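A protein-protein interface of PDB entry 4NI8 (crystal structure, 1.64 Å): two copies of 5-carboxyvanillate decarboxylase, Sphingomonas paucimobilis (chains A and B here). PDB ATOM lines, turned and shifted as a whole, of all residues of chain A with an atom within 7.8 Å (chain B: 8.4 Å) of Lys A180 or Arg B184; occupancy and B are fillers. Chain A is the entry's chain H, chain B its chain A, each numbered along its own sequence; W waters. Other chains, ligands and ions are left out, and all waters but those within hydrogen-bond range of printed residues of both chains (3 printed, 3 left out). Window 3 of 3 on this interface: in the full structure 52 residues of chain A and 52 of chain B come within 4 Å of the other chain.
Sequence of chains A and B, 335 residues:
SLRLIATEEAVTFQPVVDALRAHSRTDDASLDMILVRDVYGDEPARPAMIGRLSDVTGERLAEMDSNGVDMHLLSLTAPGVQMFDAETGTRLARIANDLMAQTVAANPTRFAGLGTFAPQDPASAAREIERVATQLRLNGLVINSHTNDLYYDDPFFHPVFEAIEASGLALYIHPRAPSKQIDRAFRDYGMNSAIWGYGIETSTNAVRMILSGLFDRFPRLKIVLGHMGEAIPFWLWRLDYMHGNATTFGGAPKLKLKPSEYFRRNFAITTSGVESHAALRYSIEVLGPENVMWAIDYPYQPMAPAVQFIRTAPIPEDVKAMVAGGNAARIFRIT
The side-chain amide oxygen of Gln B181 lies close to the backbone carbonyl oxygen of Arg A184, 3.2 Å away. NH1 of Arg A208 is in hydrogen-bond range of O of Ala B185. The side-chain amide oxygen (OE1) of Gln A181 lies close to the backbone NH (N) of Ala B185. O of Arg B184 sits close to OE1 of Gln A181, at 3.3 Å. NH2 of Arg A184 lies within hydrogen-bond range of O of Lys B180. The backbone carbonyl oxygen (O) of Lys A180 sits at hydrogen-bond distance from the guanidinium group (NH1) of Arg B184 (3.3 Å). The side-chain carboxylate (OD2) of Asp B188 lies within salt-bridge range of the guanidinium group (NH2) of Arg A208 (3.1 Å).
OG of Ser A179 lies close to N of Gln A181, 3.1 Å away. NE2 of Gln A181 sits at hydrogen-bond distance from O of Asp A149 (2.8 Å). The side-chain carboxylate (OD1) of Asp A149 is in hydrogen-bond range of the backbone NH (N) of Lys A180, 2.8 Å away. The side-chain hydroxyl of Ser B179 sits close to the backbone NH of Gln B181, at 3.1 Å.
Among the printed residues, merely in contact across the chains: Gln A181 with Gln B181, Gln A181 with Ile B182, Ile A182 with Gln B181, Ile A182 with Ile B182 and Ile A182 with Ala B185.
Pro A178 touches none of the printed residues of chain B. No residue of chain B comes within 4 Å of Ser A179. Printed residues of chain B within 4 Å of Gln A181: Gln B181, Ile B182, Arg B184 and Ala B185. Arg A187 touches none of the printed residues of chain B. Printed residues of chain A within 4 Å of Lys B180: Arg A184 (2.8 Å). Printed residues of chain A within 4 Å of Gln B181: Gln A181 (3.9 Å), Ile A182 (3.8 Å) and Arg A184 (3.2 Å). Of the printed residues of chain A, Ala B185 touches Gln A181, Ile A182 and Arg A208. The nearest residue of chain B that does not touch Lys A180 is Gln B181 (5.7 Å). The nearest printed residue of chain A that does not touch Arg B184 is Arg A208 (4.7 Å).
Printed residues of chain B that touch a printed residue of chain A: Lys B180, Gln B181, Ile B182, Arg B184, Ala B185 and Asp B188. Hydrophobic or aromatic side chains of chain B within 4 Å of the printed part of chain A: Ile B182 and Ala B185. Of the 21 printed residues of chain A, 5 touch a printed residue of chain B. Hydrophobic or aromatic side chains of chain A within 4 Å of the printed part of chain B: Ile A182. Among the printed residues, 12 pairs touch across the chains.
Lys A180 touches Arg B184, and with the chains exchanged Arg A184 touches Lys B180. Gln A181 touches its own counterpart, Gln B181. Gln A181 touches Ile B182, and with the chains exchanged Ile A182 touches Gln B181. Ile B182 touches its own counterpart, Ile A182. Positions printed for both chains: 31, 178, 179, 180, 181, 182, 183, 184 and 187.
Water W2 lies within hydrogen-bond range of O of Gln A181 (2.8 Å), N of Arg B184 (3.1 Å), O of Lys B180 (3.3 Å) and N of Asp B183 (3.3 Å). Water W1 bridges the side-chain amide oxygen (OE1) of Gln A181 (2.8 Å) and the backbone carbonyl oxygen (O) of Arg B184 (3.2 Å). Water W3 bridges OE1 of Gln B181 (2.8 Å) and O of Arg A184 (3.0 Å).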
ATOM      1  N   ASP A  27      -8.521  28.333  32.366  1.00  0.00           N
ATOM      2  CA  ASP A  27      -8.394  27.019  32.995  1.00  0.00           C
ATOM      3  C   ASP A  27      -9.543  26.072  32.657  1.00  0.00           C
ATOM      4  O   ASP A  27      -9.827  25.145  33.418  1.00  0.00           O
ATOM      5  CB  ASP A  27      -8.262  27.157  34.512  1.00  0.00           C
ATOM      6  CG  ASP A  27      -9.525  27.680  35.166  1.00  0.00           C
ATOM      7  OD1 ASP A  27     -10.476  28.052  34.445  1.00  0.00           O
ATOM      8  OD2 ASP A  27      -9.561  27.733  36.411  1.00  0.00           O
ATOM      9  N   ASP A  28     -10.200  26.317  31.528  1.00  0.00           N
ATOM     10  CA  ASP A  28     -11.249  25.435  31.023  1.00  0.00           C
ATOM     11  C   ASP A  28     -10.763  23.977  31.066  1.00  0.00           C
ATOM     12  O   ASP A  28      -9.668  23.676  30.586  1.00  0.00           O
ATOM     13  CB  ASP A  28     -11.592  25.852  29.587  1.00  0.00           C
ATOM     14  CG  ASP A  28     -12.862  25.196  29.054  1.00  0.00           C
ATOM     15  OD1 ASP A  28     -13.267  24.130  29.564  1.00  0.00           O
ATOM     16  OD2 ASP A  28     -13.446  25.748  28.096  1.00  0.00           O
ATOM     17  N   ALA A  29     -11.572  23.080  31.636  1.00  0.00           N
ATOM     18  CA  ALA A  29     -11.182  21.668  31.757  1.00  0.00           C
ATOM     19  C   ALA A  29     -11.606  20.792  30.577  1.00  0.00           C
ATOM     20  O   ALA A  29     -11.348  19.581  30.569  1.00  0.00           O
ATOM     21  CB  ALA A  29     -11.711  21.072  33.068  1.00  0.00           C
ATOM     22  N   SER A  30     -12.255  21.393  29.585  1.00  0.00           N
ATOM     23  CA  SER A  30     -12.655  20.656  28.395  1.00  0.00           C
ATOM     24  C   SER A  30     -11.464  20.001  27.709  1.00  0.00           C
ATOM     25  O   SER A  30     -10.394  20.606  27.575  1.00  0.00           O
ATOM     26  CB  SER A  30     -13.358  21.582  27.407  1.00  0.00           C
ATOM     27  OG  SER A  30     -13.664  20.905  26.197  1.00  0.00           O
ATOM     28  N   LEU A  31     -11.656  18.766  27.260  1.00  0.00           N
ATOM     29  CA  LEU A  31     -10.596  18.048  26.562  1.00  0.00           C
ATOM     30  C   LEU A  31     -10.195  18.742  25.255  1.00  0.00           C
ATOM     31  O   LEU A  31      -9.100  18.516  24.735  1.00  0.00           O
ATOM     32  CB  LEU A  31     -11.007  16.594  26.305  1.00  0.00           C
ATOM     33  CG  LEU A  31      -9.858  15.631  25.991  1.00  0.00           C
ATOM     34  CD1 LEU A  31      -8.865  15.586  27.154  1.00  0.00           C
ATOM     35  CD2 LEU A  31     -10.398  14.235  25.684  1.00  0.00           C
ATOM     36  N   HIS A 146     -20.813  17.530  20.951  1.00  0.00           N
ATOM     37  CA  HIS A 146     -21.521  18.004  22.148  1.00  0.00           C
ATOM     38  C   HIS A 146     -21.460  19.517  22.353  1.00  0.00           C
ATOM     39  O   HIS A 146     -20.567  20.196  21.833  1.00  0.00           O
ATOM     40  CB  HIS A 146     -20.978  17.301  23.401  1.00  0.00           C
ATOM     41  CG  HIS A 146     -19.697  17.880  23.921  1.00  0.00           C
ATOM     42  ND1 HIS A 146     -19.662  18.938  24.806  1.00  0.00           N
ATOM     43  CD2 HIS A 146     -18.407  17.542  23.689  1.00  0.00           C
ATOM     44  CE1 HIS A 146     -18.406  19.228  25.096  1.00  0.00           C
ATOM     45  NE2 HIS A 146     -17.624  18.401  24.424  1.00  0.00           N
ATOM     46  N   ASN A 148     -21.782  21.976  25.916  1.00  0.00           N
ATOM     47  CA  ASN A 148     -21.891  21.991  27.377  1.00  0.00           C
ATOM     48  C   ASN A 148     -21.911  20.584  27.962  1.00  0.00           C
ATOM     49  O   ASN A 148     -22.531  20.356  28.999  1.00  0.00           O
ATOM     50  CB  ASN A 148     -23.129  22.763  27.844  1.00  0.00           C
ATOM     51  CG  ASN A 148     -23.119  24.227  27.403  1.00  0.00           C
ATOM     52  OD1 ASN A 148     -22.063  24.845  27.255  1.00  0.00           O
ATOM     53  ND2 ASN A 148     -24.308  24.789  27.209  1.00  0.00           N
ATOM     54  N   ASP A 149     -21.242  19.653  27.282  1.00  0.00           N
ATOM     55  CA  ASP A 149     -21.157  18.268  27.729  1.00  0.00           C
ATOM     56  C   ASP A 149     -22.517  17.565  27.775  1.00  0.00           C
ATOM     57  O   ASP A 149     -22.744  16.673  28.583  1.00  0.00           O
ATOM     58  CB  ASP A 149     -20.399  18.174  29.058  1.00  0.00           C
ATOM     59  CG  ASP A 149     -19.030  18.815  28.975  1.00  0.00           C
ATOM     60  OD1 ASP A 149     -18.175  18.280  28.235  1.00  0.00           O
ATOM     61  OD2 ASP A 149     -18.832  19.873  29.606  1.00  0.00           O
ATOM     62  N   LEU A 150     -23.400  17.981  26.873  1.00  0.00           N
ATOM     63  CA  LEU A 150     -24.690  17.330  26.660  1.00  0.00           C
ATOM     64  C   LEU A 150     -24.784  16.889  25.211  1.00  0.00           C
ATOM     65  O   LEU A 150     -24.191  17.508  24.333  1.00  0.00           O
ATOM     66  CB  LEU A 150     -25.835  18.294  26.968  1.00  0.00           C
ATOM     67  CG  LEU A 150     -25.954  18.815  28.398  1.00  0.00           C
ATOM     68  CD1 LEU A 150     -27.096  19.809  28.465  1.00  0.00           C
ATOM     69  CD2 LEU A 150     -26.171  17.680  29.388  1.00  0.00           C
ATOM     70  N   TYR A 151     -25.538  15.817  24.960  1.00  0.00           N
ATOM     71  CA  TYR A 151     -25.687  15.298  23.610  1.00  0.00           C
ATOM     72  C   TYR A 151     -27.053  15.685  23.058  1.00  0.00           C
ATOM     73  O   TYR A 151     -27.915  16.144  23.805  1.00  0.00           O
ATOM     74  CB  TYR A 151     -25.458  13.784  23.601  1.00  0.00           C
ATOM     75  CG  TYR A 151     -24.031  13.429  23.968  1.00  0.00           C
ATOM     76  CD1 TYR A 151     -22.990  13.693  23.082  1.00  0.00           C
ATOM     77  CD2 TYR A 151     -23.722  12.840  25.192  1.00  0.00           C
ATOM     78  CE1 TYR A 151     -21.673  13.382  23.405  1.00  0.00           C
ATOM     79  CE2 TYR A 151     -22.401  12.528  25.532  1.00  0.00           C
ATOM     80  CZ  TYR A 151     -21.382  12.803  24.621  1.00  0.00           C
ATOM     81  OH  TYR A 151     -20.073  12.503  24.936  1.00  0.00           O
ATOM     82  N   ALA A 177     -13.428  16.975  20.756  1.00  0.00           N
ATOM     83  CA  ALA A 177     -12.913  16.025  21.737  1.00  0.00           C
ATOM     84  C   ALA A 177     -14.043  15.478  22.615  1.00  0.00           C
ATOM     85  O   ALA A 177     -15.052  16.156  22.832  1.00  0.00           O
ATOM     86  CB  ALA A 177     -11.811  16.663  22.597  1.00  0.00           C
ATOM     87  N   PRO A 178     -13.886  14.236  23.092  1.00  0.00           N
ATOM     88  CA  PRO A 178     -14.816  13.629  24.046  1.00  0.00           C
ATOM     89  C   PRO A 178     -15.255  14.596  25.142  1.00  0.00           C
ATOM     90  O   PRO A 178     -14.415  15.298  25.712  1.00  0.00           O
ATOM     91  CB  PRO A 178     -13.980  12.500  24.641  1.00  0.00           C
ATOM     92  CG  PRO A 178     -13.178  12.035  23.461  1.00  0.00           C
ATOM     93  CD  PRO A 178     -12.856  13.272  22.656  1.00  0.00           C
ATOM     94  N   SER A 179     -16.555  14.616  25.416  1.00  0.00           N
ATOM     95  CA  SER A 179     -17.146  15.470  26.448  1.00  0.00           C
ATOM     96  C   SER A 179     -16.705  15.016  27.830  1.00  0.00           C
ATOM     97  O   SER A 179     -16.094  13.954  27.985  1.00  0.00           O
ATOM     98  CB  SER A 179     -18.674  15.396  26.388  1.00  0.00           C
ATOM     99  OG  SER A 179     -19.129  14.201  27.006  1.00  0.00           O
ATOM    100  N   LYS A 180     -17.063  15.797  28.843  1.00  0.00           N
ATOM    101  CA  LYS A 180     -16.682  15.472  30.213  1.00  0.00           C
ATOM    102  C   LYS A 180     -17.336  14.183  30.710  1.00  0.00           C
ATOM    103  O   LYS A 180     -16.897  13.612  31.709  1.00  0.00           O
ATOM    104  CB  LYS A 180     -17.002  16.635  31.154  1.00  0.00           C
ATOM    105  CG  LYS A 180     -16.118  17.835  30.911  1.00  0.00           C
ATOM    106  CD  LYS A 180     -16.417  18.961  31.869  1.00  0.00           C
ATOM    107  CE  LYS A 180     -15.606  20.204  31.508  1.00  0.00           C
ATOM    108  NZ  LYS A 180     -15.666  21.213  32.601  1.00  0.00           N
ATOM    109  N   GLN A 181     -18.383  13.735  30.021  1.00  0.00           N
ATOM    110  CA  GLN A 181     -19.036  12.481  30.390  1.00  0.00           C
ATOM    111  C   GLN A 181     -18.111  11.285  30.143  1.00  0.00           C
ATOM    112  O   GLN A 181     -18.240  10.252  30.802  1.00  0.00           O
ATOM    113  CB  GLN A 181     -20.345  12.282  29.613  1.00  0.00           C
ATOM    114  CG  GLN A 181     -21.405  13.369  29.847  1.00  0.00           C
ATOM    115  CD  GLN A 181     -22.784  12.974  29.318  1.00  0.00           C
ATOM    116  OE1 GLN A 181     -23.203  11.826  29.455  1.00  0.00           O
ATOM    117  NE2 GLN A 181     -23.493  13.928  28.716  1.00  0.00           N
ATOM    118  N   ILE A 182     -17.185  11.420  29.197  1.00  0.00           N
ATOM    119  CA  ILE A 182     -16.365  10.277  28.790  1.00  0.00           C
ATOM    120  C   ILE A 182     -14.864  10.579  28.692  1.00  0.00           C
ATOM    121  O   ILE A 182     -14.078   9.671  28.430  1.00  0.00           O
ATOM    122  CB  ILE A 182     -16.801   9.721  27.402  1.00  0.00           C
ATOM    123  CG1 ILE A 182     -16.709  10.814  26.334  1.00  0.00           C
ATOM    124  CG2 ILE A 182     -18.209   9.147  27.454  1.00  0.00           C
ATOM    125  CD1 ILE A 182     -16.961  10.303  24.920  1.00  0.00           C
ATOM    126  N   ASP A 183     -14.461  11.833  28.890  1.00  0.00           N
ATOM    127  CA  ASP A 183     -13.072  12.229  28.581  1.00  0.00           C
ATOM    128  C   ASP A 183     -11.968  11.546  29.398  1.00  0.00           C
ATOM    129  O   ASP A 183     -10.816  11.492  28.956  1.00  0.00           O
ATOM    130  CB  ASP A 183     -12.869  13.766  28.557  1.00  0.00           C
ATOM    131  CG  ASP A 183     -13.052  14.431  29.922  1.00  0.00           C
ATOM    132  OD1 ASP A 183     -12.873  13.771  30.969  1.00  0.00           O
ATOM    133  OD2 ASP A 183     -13.354  15.650  29.948  1.00  0.00           O
ATOM    134  N   ARG A 184     -12.305  11.025  30.573  1.00  0.00           N
ATOM    135  CA  ARG A 184     -11.291  10.383  31.414  1.00  0.00           C
ATOM    136  C   ARG A 184     -10.505   9.269  30.704  1.00  0.00           C
ATOM    137  O   ARG A 184      -9.325   9.065  30.986  1.00  0.00           O
ATOM    138  CB  ARG A 184     -11.904   9.876  32.719  1.00  0.00           C
ATOM    139  CG  ARG A 184     -11.938  10.949  33.797  1.00  0.00           C
ATOM    140  CD  ARG A 184     -13.256  10.964  34.544  1.00  0.00           C
ATOM    141  NE  ARG A 184     -13.425   9.788  35.387  1.00  0.00           N
ATOM    142  CZ  ARG A 184     -14.595   9.387  35.874  1.00  0.00           C
ATOM    143  NH1 ARG A 184     -15.703  10.064  35.587  1.00  0.00           N
ATOM    144  NH2 ARG A 184     -14.659   8.303  36.640  1.00  0.00           N
ATOM    145  N   ARG A 187      -7.325  10.535  27.784  1.00  0.00           N
ATOM    146  CA  ARG A 187      -6.282  11.465  28.199  1.00  0.00           C
ATOM    147  C   ARG A 187      -4.888  11.029  27.785  1.00  0.00           C
ATOM    148  O   ARG A 187      -3.937  11.804  27.901  1.00  0.00           O
ATOM    149  CB  ARG A 187      -6.313  11.640  29.716  1.00  0.00           C
ATOM    150  CG  ARG A 187      -7.608  12.225  30.250  1.00  0.00           C
ATOM    151  CD  ARG A 187      -7.688  13.711  30.001  1.00  0.00           C
ATOM    152  NE  ARG A 187      -8.617  14.341  30.934  1.00  0.00           N
ATOM    153  CZ  ARG A 187      -8.794  15.653  31.049  1.00  0.00           C
ATOM    154  NH1 ARG A 187      -8.107  16.491  30.285  1.00  0.00           N
ATOM    155  NH2 ARG A 187      -9.665  16.124  31.934  1.00  0.00           N
ATOM    156  N   GLU A 201     -16.783  10.050  20.477  1.00  0.00           N
ATOM    157  CA  GLU A 201     -17.610  11.176  20.903  1.00  0.00           C
ATOM    158  C   GLU A 201     -18.761  11.410  19.913  1.00  0.00           C
ATOM    159  O   GLU A 201     -19.935  11.501  20.306  1.00  0.00           O
ATOM    160  CB  GLU A 201     -16.712  12.413  21.038  1.00  0.00           C
ATOM    161  CG  GLU A 201     -17.404  13.763  20.979  1.00  0.00           C
ATOM    162  CD  GLU A 201     -18.331  14.029  22.138  1.00  0.00           C
ATOM    163  OE1 GLU A 201     -18.196  13.384  23.205  1.00  0.00           O
ATOM    164  OE2 GLU A 201     -19.205  14.910  21.971  1.00  0.00           O
ATOM    165  N   ARG A 208     -27.227   8.194  20.406  1.00  0.00           N
ATOM    166  CA  ARG A 208     -28.189   8.744  21.374  1.00  0.00           C
ATOM    167  C   ARG A 208     -29.337   9.450  20.643  1.00  0.00           C
ATOM    168  O   ARG A 208     -30.500   9.281  20.997  1.00  0.00           O
ATOM    169  CB  ARG A 208     -27.513   9.717  22.358  1.00  0.00           C
ATOM    170  CG  ARG A 208     -26.516   9.059  23.317  1.00  0.00           C
ATOM    171  CD  ARG A 208     -25.869  10.081  24.246  1.00  0.00           C
ATOM    172  NE  ARG A 208     -26.871  10.706  25.117  1.00  0.00           N
ATOM    173  CZ  ARG A 208     -27.062  10.400  26.395  1.00  0.00           C
ATOM    174  NH1 ARG A 208     -26.299   9.495  26.998  1.00  0.00           N
ATOM    175  NH2 ARG A 208     -28.016  11.010  27.080  1.00  0.00           N
ATOM    176  N   LEU B  31     -21.689   0.170  36.291  1.00  0.00           N
ATOM    177  CA  LEU B  31     -22.779   0.102  35.325  1.00  0.00           C
ATOM    178  C   LEU B  31     -23.216  -1.343  35.045  1.00  0.00           C
ATOM    179  O   LEU B  31     -24.342  -1.582  34.591  1.00  0.00           O
ATOM    180  CB  LEU B  31     -22.384   0.837  34.037  1.00  0.00           C
ATOM    181  CG  LEU B  31     -23.480   1.127  33.010  1.00  0.00           C
ATOM    182  CD1 LEU B  31     -24.551   2.026  33.623  1.00  0.00           C
ATOM    183  CD2 LEU B  31     -22.868   1.769  31.769  1.00  0.00           C
ATOM    184  N   PRO B 178     -19.602  -0.238  30.118  1.00  0.00           N
ATOM    185  CA  PRO B 178     -18.639   0.865  30.239  1.00  0.00           C
ATOM    186  C   PRO B 178     -18.162   1.093  31.673  1.00  0.00           C
ATOM    187  O   PRO B 178     -18.973   1.088  32.605  1.00  0.00           O
ATOM    188  CB  PRO B 178     -19.456   2.058  29.763  1.00  0.00           C
ATOM    189  CG  PRO B 178     -20.273   1.447  28.615  1.00  0.00           C
ATOM    190  CD  PRO B 178     -20.607   0.027  29.072  1.00  0.00           C
ATOM    191  N   SER B 179     -16.851   1.293  31.826  1.00  0.00           N
ATOM    192  CA  SER B 179     -16.237   1.576  33.119  1.00  0.00           C
ATOM    193  C   SER B 179     -16.676   2.932  33.655  1.00  0.00           C
ATOM    194  O   SER B 179     -17.324   3.721  32.956  1.00  0.00           O
ATOM    195  CB  SER B 179     -14.716   1.589  32.980  1.00  0.00           C
ATOM    196  OG  SER B 179     -14.281   2.822  32.422  1.00  0.00           O
ATOM    197  N   LYS B 180     -16.294   3.218  34.890  1.00  0.00           N
ATOM    198  CA  LYS B 180     -16.642   4.492  35.500  1.00  0.00           C
ATOM    199  C   LYS B 180     -15.982   5.661  34.778  1.00  0.00           C
ATOM    200  O   LYS B 180     -16.392   6.806  34.952  1.00  0.00           O
ATOM    201  CB  LYS B 180     -16.257   4.501  36.979  1.00  0.00           C
ATOM    202  CG  LYS B 180     -17.125   3.570  37.815  1.00  0.00           C
ATOM    203  CD  LYS B 180     -16.797   3.675  39.295  1.00  0.00           C
ATOM    204  CE  LYS B 180     -17.652   2.677  40.090  1.00  0.00           C
ATOM    205  NZ  LYS B 180     -17.404   2.759  41.558  1.00  0.00           N
ATOM    206  N   GLN B 181     -14.972   5.377  33.964  1.00  0.00           N
ATOM    207  CA  GLN B 181     -14.315   6.449  33.219  1.00  0.00           C
ATOM    208  C   GLN B 181     -15.251   7.037  32.167  1.00  0.00           C
ATOM    209  O   GLN B 181     -15.112   8.202  31.771  1.00  0.00           O
ATOM    210  CB  GLN B 181     -13.040   5.941  32.544  1.00  0.00           C
ATOM    211  CG  GLN B 181     -11.966   5.449  33.511  1.00  0.00           C
ATOM    212  CD  GLN B 181     -10.611   5.305  32.835  1.00  0.00           C
ATOM    213  OE1 GLN B 181     -10.240   6.126  31.998  1.00  0.00           O
ATOM    214  NE2 GLN B 181      -9.868   4.263  33.191  1.00  0.00           N
ATOM    215  N   ILE B 182     -16.207   6.232  31.717  1.00  0.00           N
ATOM    216  CA  ILE B 182     -17.022   6.622  30.568  1.00  0.00           C
ATOM    217  C   ILE B 182     -18.513   6.390  30.765  1.00  0.00           C
ATOM    218  O   ILE B 182     -19.315   6.791  29.922  1.00  0.00           O
ATOM    219  CB  ILE B 182     -16.580   5.889  29.269  1.00  0.00           C
ATOM    220  CG1 ILE B 182     -16.595   4.365  29.439  1.00  0.00           C
ATOM    221  CG2 ILE B 182     -15.187   6.345  28.842  1.00  0.00           C
ATOM    222  CD1 ILE B 182     -16.500   3.603  28.111  1.00  0.00           C
ATOM    223  N   ASP B 183     -18.893   5.760  31.869  1.00  0.00           N
ATOM    224  CA  ASP B 183     -20.278   5.298  31.981  1.00  0.00           C
ATOM    225  C   ASP B 183     -21.363   6.376  32.021  1.00  0.00           C
ATOM    226  O   ASP B 183     -22.526   6.063  31.821  1.00  0.00           O
ATOM    227  CB  ASP B 183     -20.472   4.282  33.126  1.00  0.00           C
ATOM    228  CG  ASP B 183     -20.257   4.879  34.501  1.00  0.00           C
ATOM    229  OD1 ASP B 183     -20.332   6.121  34.661  1.00  0.00           O
ATOM    230  OD2 ASP B 183     -20.021   4.091  35.444  1.00  0.00           O
ATOM    231  N   ARG B 184     -21.002   7.634  32.265  1.00  0.00           N
ATOM    232  CA  ARG B 184     -22.020   8.685  32.354  1.00  0.00           C
ATOM    233  C   ARG B 184     -22.862   8.802  31.075  1.00  0.00           C
ATOM    234  O   ARG B 184     -24.054   9.135  31.133  1.00  0.00           O
ATOM    235  CB  ARG B 184     -21.391  10.038  32.721  1.00  0.00           C
ATOM    236  CG  ARG B 184     -21.045  10.183  34.205  1.00  0.00           C
ATOM    237  CD  ARG B 184     -20.123  11.381  34.462  1.00  0.00           C
ATOM    238  NE  ARG B 184     -20.643  12.626  33.895  1.00  0.00           N
ATOM    239  CZ  ARG B 184     -19.972  13.777  33.879  1.00  0.00           C
ATOM    240  NH1 ARG B 184     -18.752  13.844  34.398  1.00  0.00           N
ATOM    241  NH2 ARG B 184     -20.514  14.862  33.337  1.00  0.00           N
ATOM    242  N   ALA B 185     -22.240   8.513  29.934  1.00  0.00           N
ATOM    243  CA  ALA B 185     -22.892   8.670  28.639  1.00  0.00           C
ATOM    244  C   ALA B 185     -23.692   7.448  28.219  1.00  0.00           C
ATOM    245  O   ALA B 185     -24.324   7.457  27.155  1.00  0.00           O
ATOM    246  CB  ALA B 185     -21.861   9.015  27.562  1.00  0.00           C
ATOM    247  N   PHE B 186     -23.679   6.400  29.050  1.00  0.00           N
ATOM    248  CA  PHE B 186     -24.339   5.145  28.705  1.00  0.00           C
ATOM    249  C   PHE B 186     -25.457   4.741  29.668  1.00  0.00           C
ATOM    250  O   PHE B 186     -25.765   3.552  29.801  1.00  0.00           O
ATOM    251  CB  PHE B 186     -23.302   4.022  28.568  1.00  0.00           C
ATOM    252  CG  PHE B 186     -22.227   4.337  27.563  1.00  0.00           C
ATOM    253  CD1 PHE B 186     -21.136   5.115  27.927  1.00  0.00           C
ATOM    254  CD2 PHE B 186     -22.327   3.897  26.256  1.00  0.00           C
ATOM    255  CE1 PHE B 186     -20.156   5.441  26.999  1.00  0.00           C
ATOM    256  CE2 PHE B 186     -21.356   4.205  25.330  1.00  0.00           C
ATOM    257  CZ  PHE B 186     -20.264   4.983  25.701  1.00  0.00           C
ATOM    258  N   ARG B 187     -26.080   5.724  30.311  1.00  0.00           N
ATOM    259  CA  ARG B 187     -27.123   5.460  31.299  1.00  0.00           C
ATOM    260  C   ARG B 187     -28.534   5.522  30.715  1.00  0.00           C
ATOM    261  O   ARG B 187     -29.515   5.285  31.430  1.00  0.00           O
ATOM    262  CB  ARG B 187     -27.005   6.453  32.461  1.00  0.00           C
ATOM    263  CG  ARG B 187     -25.760   6.274  33.324  1.00  0.00           C
ATOM    264  CD  ARG B 187     -26.034   5.322  34.480  1.00  0.00           C
ATOM    265  NE  ARG B 187     -24.842   5.048  35.284  1.00  0.00           N
ATOM    266  CZ  ARG B 187     -24.802   4.176  36.288  1.00  0.00           C
ATOM    267  NH1 ARG B 187     -25.888   3.490  36.622  1.00  0.00           N
ATOM    268  NH2 ARG B 187     -23.672   3.986  36.958  1.00  0.00           N
ATOM    269  N   ASP B 188     -28.645   5.844  29.427  1.00  0.00           N
ATOM    270  CA  ASP B 188     -29.956   6.040  28.809  1.00  0.00           C
ATOM    271  C   ASP B 188     -30.183   5.106  27.626  1.00  0.00           C
ATOM    272  O   ASP B 188     -29.237   4.648  26.996  1.00  0.00           O
ATOM    273  CB  ASP B 188     -30.120   7.492  28.348  1.00  0.00           C
ATOM    274  CG  ASP B 188     -30.014   8.483  29.492  1.00  0.00           C
ATOM    275  OD1 ASP B 188     -30.878   8.440  30.385  1.00  0.00           O
ATOM    276  OD2 ASP B 188     -29.079   9.312  29.494  1.00  0.00           O
HETATM  277  O   HOH W   1     -25.876  11.690  30.352  1.00  0.00           O
HETATM  278  O   HOH W   2     -18.297   8.755  33.173  1.00  0.00           O
HETATM  279  O   HOH W   3      -7.510   6.900  32.118  1.00  0.00           O
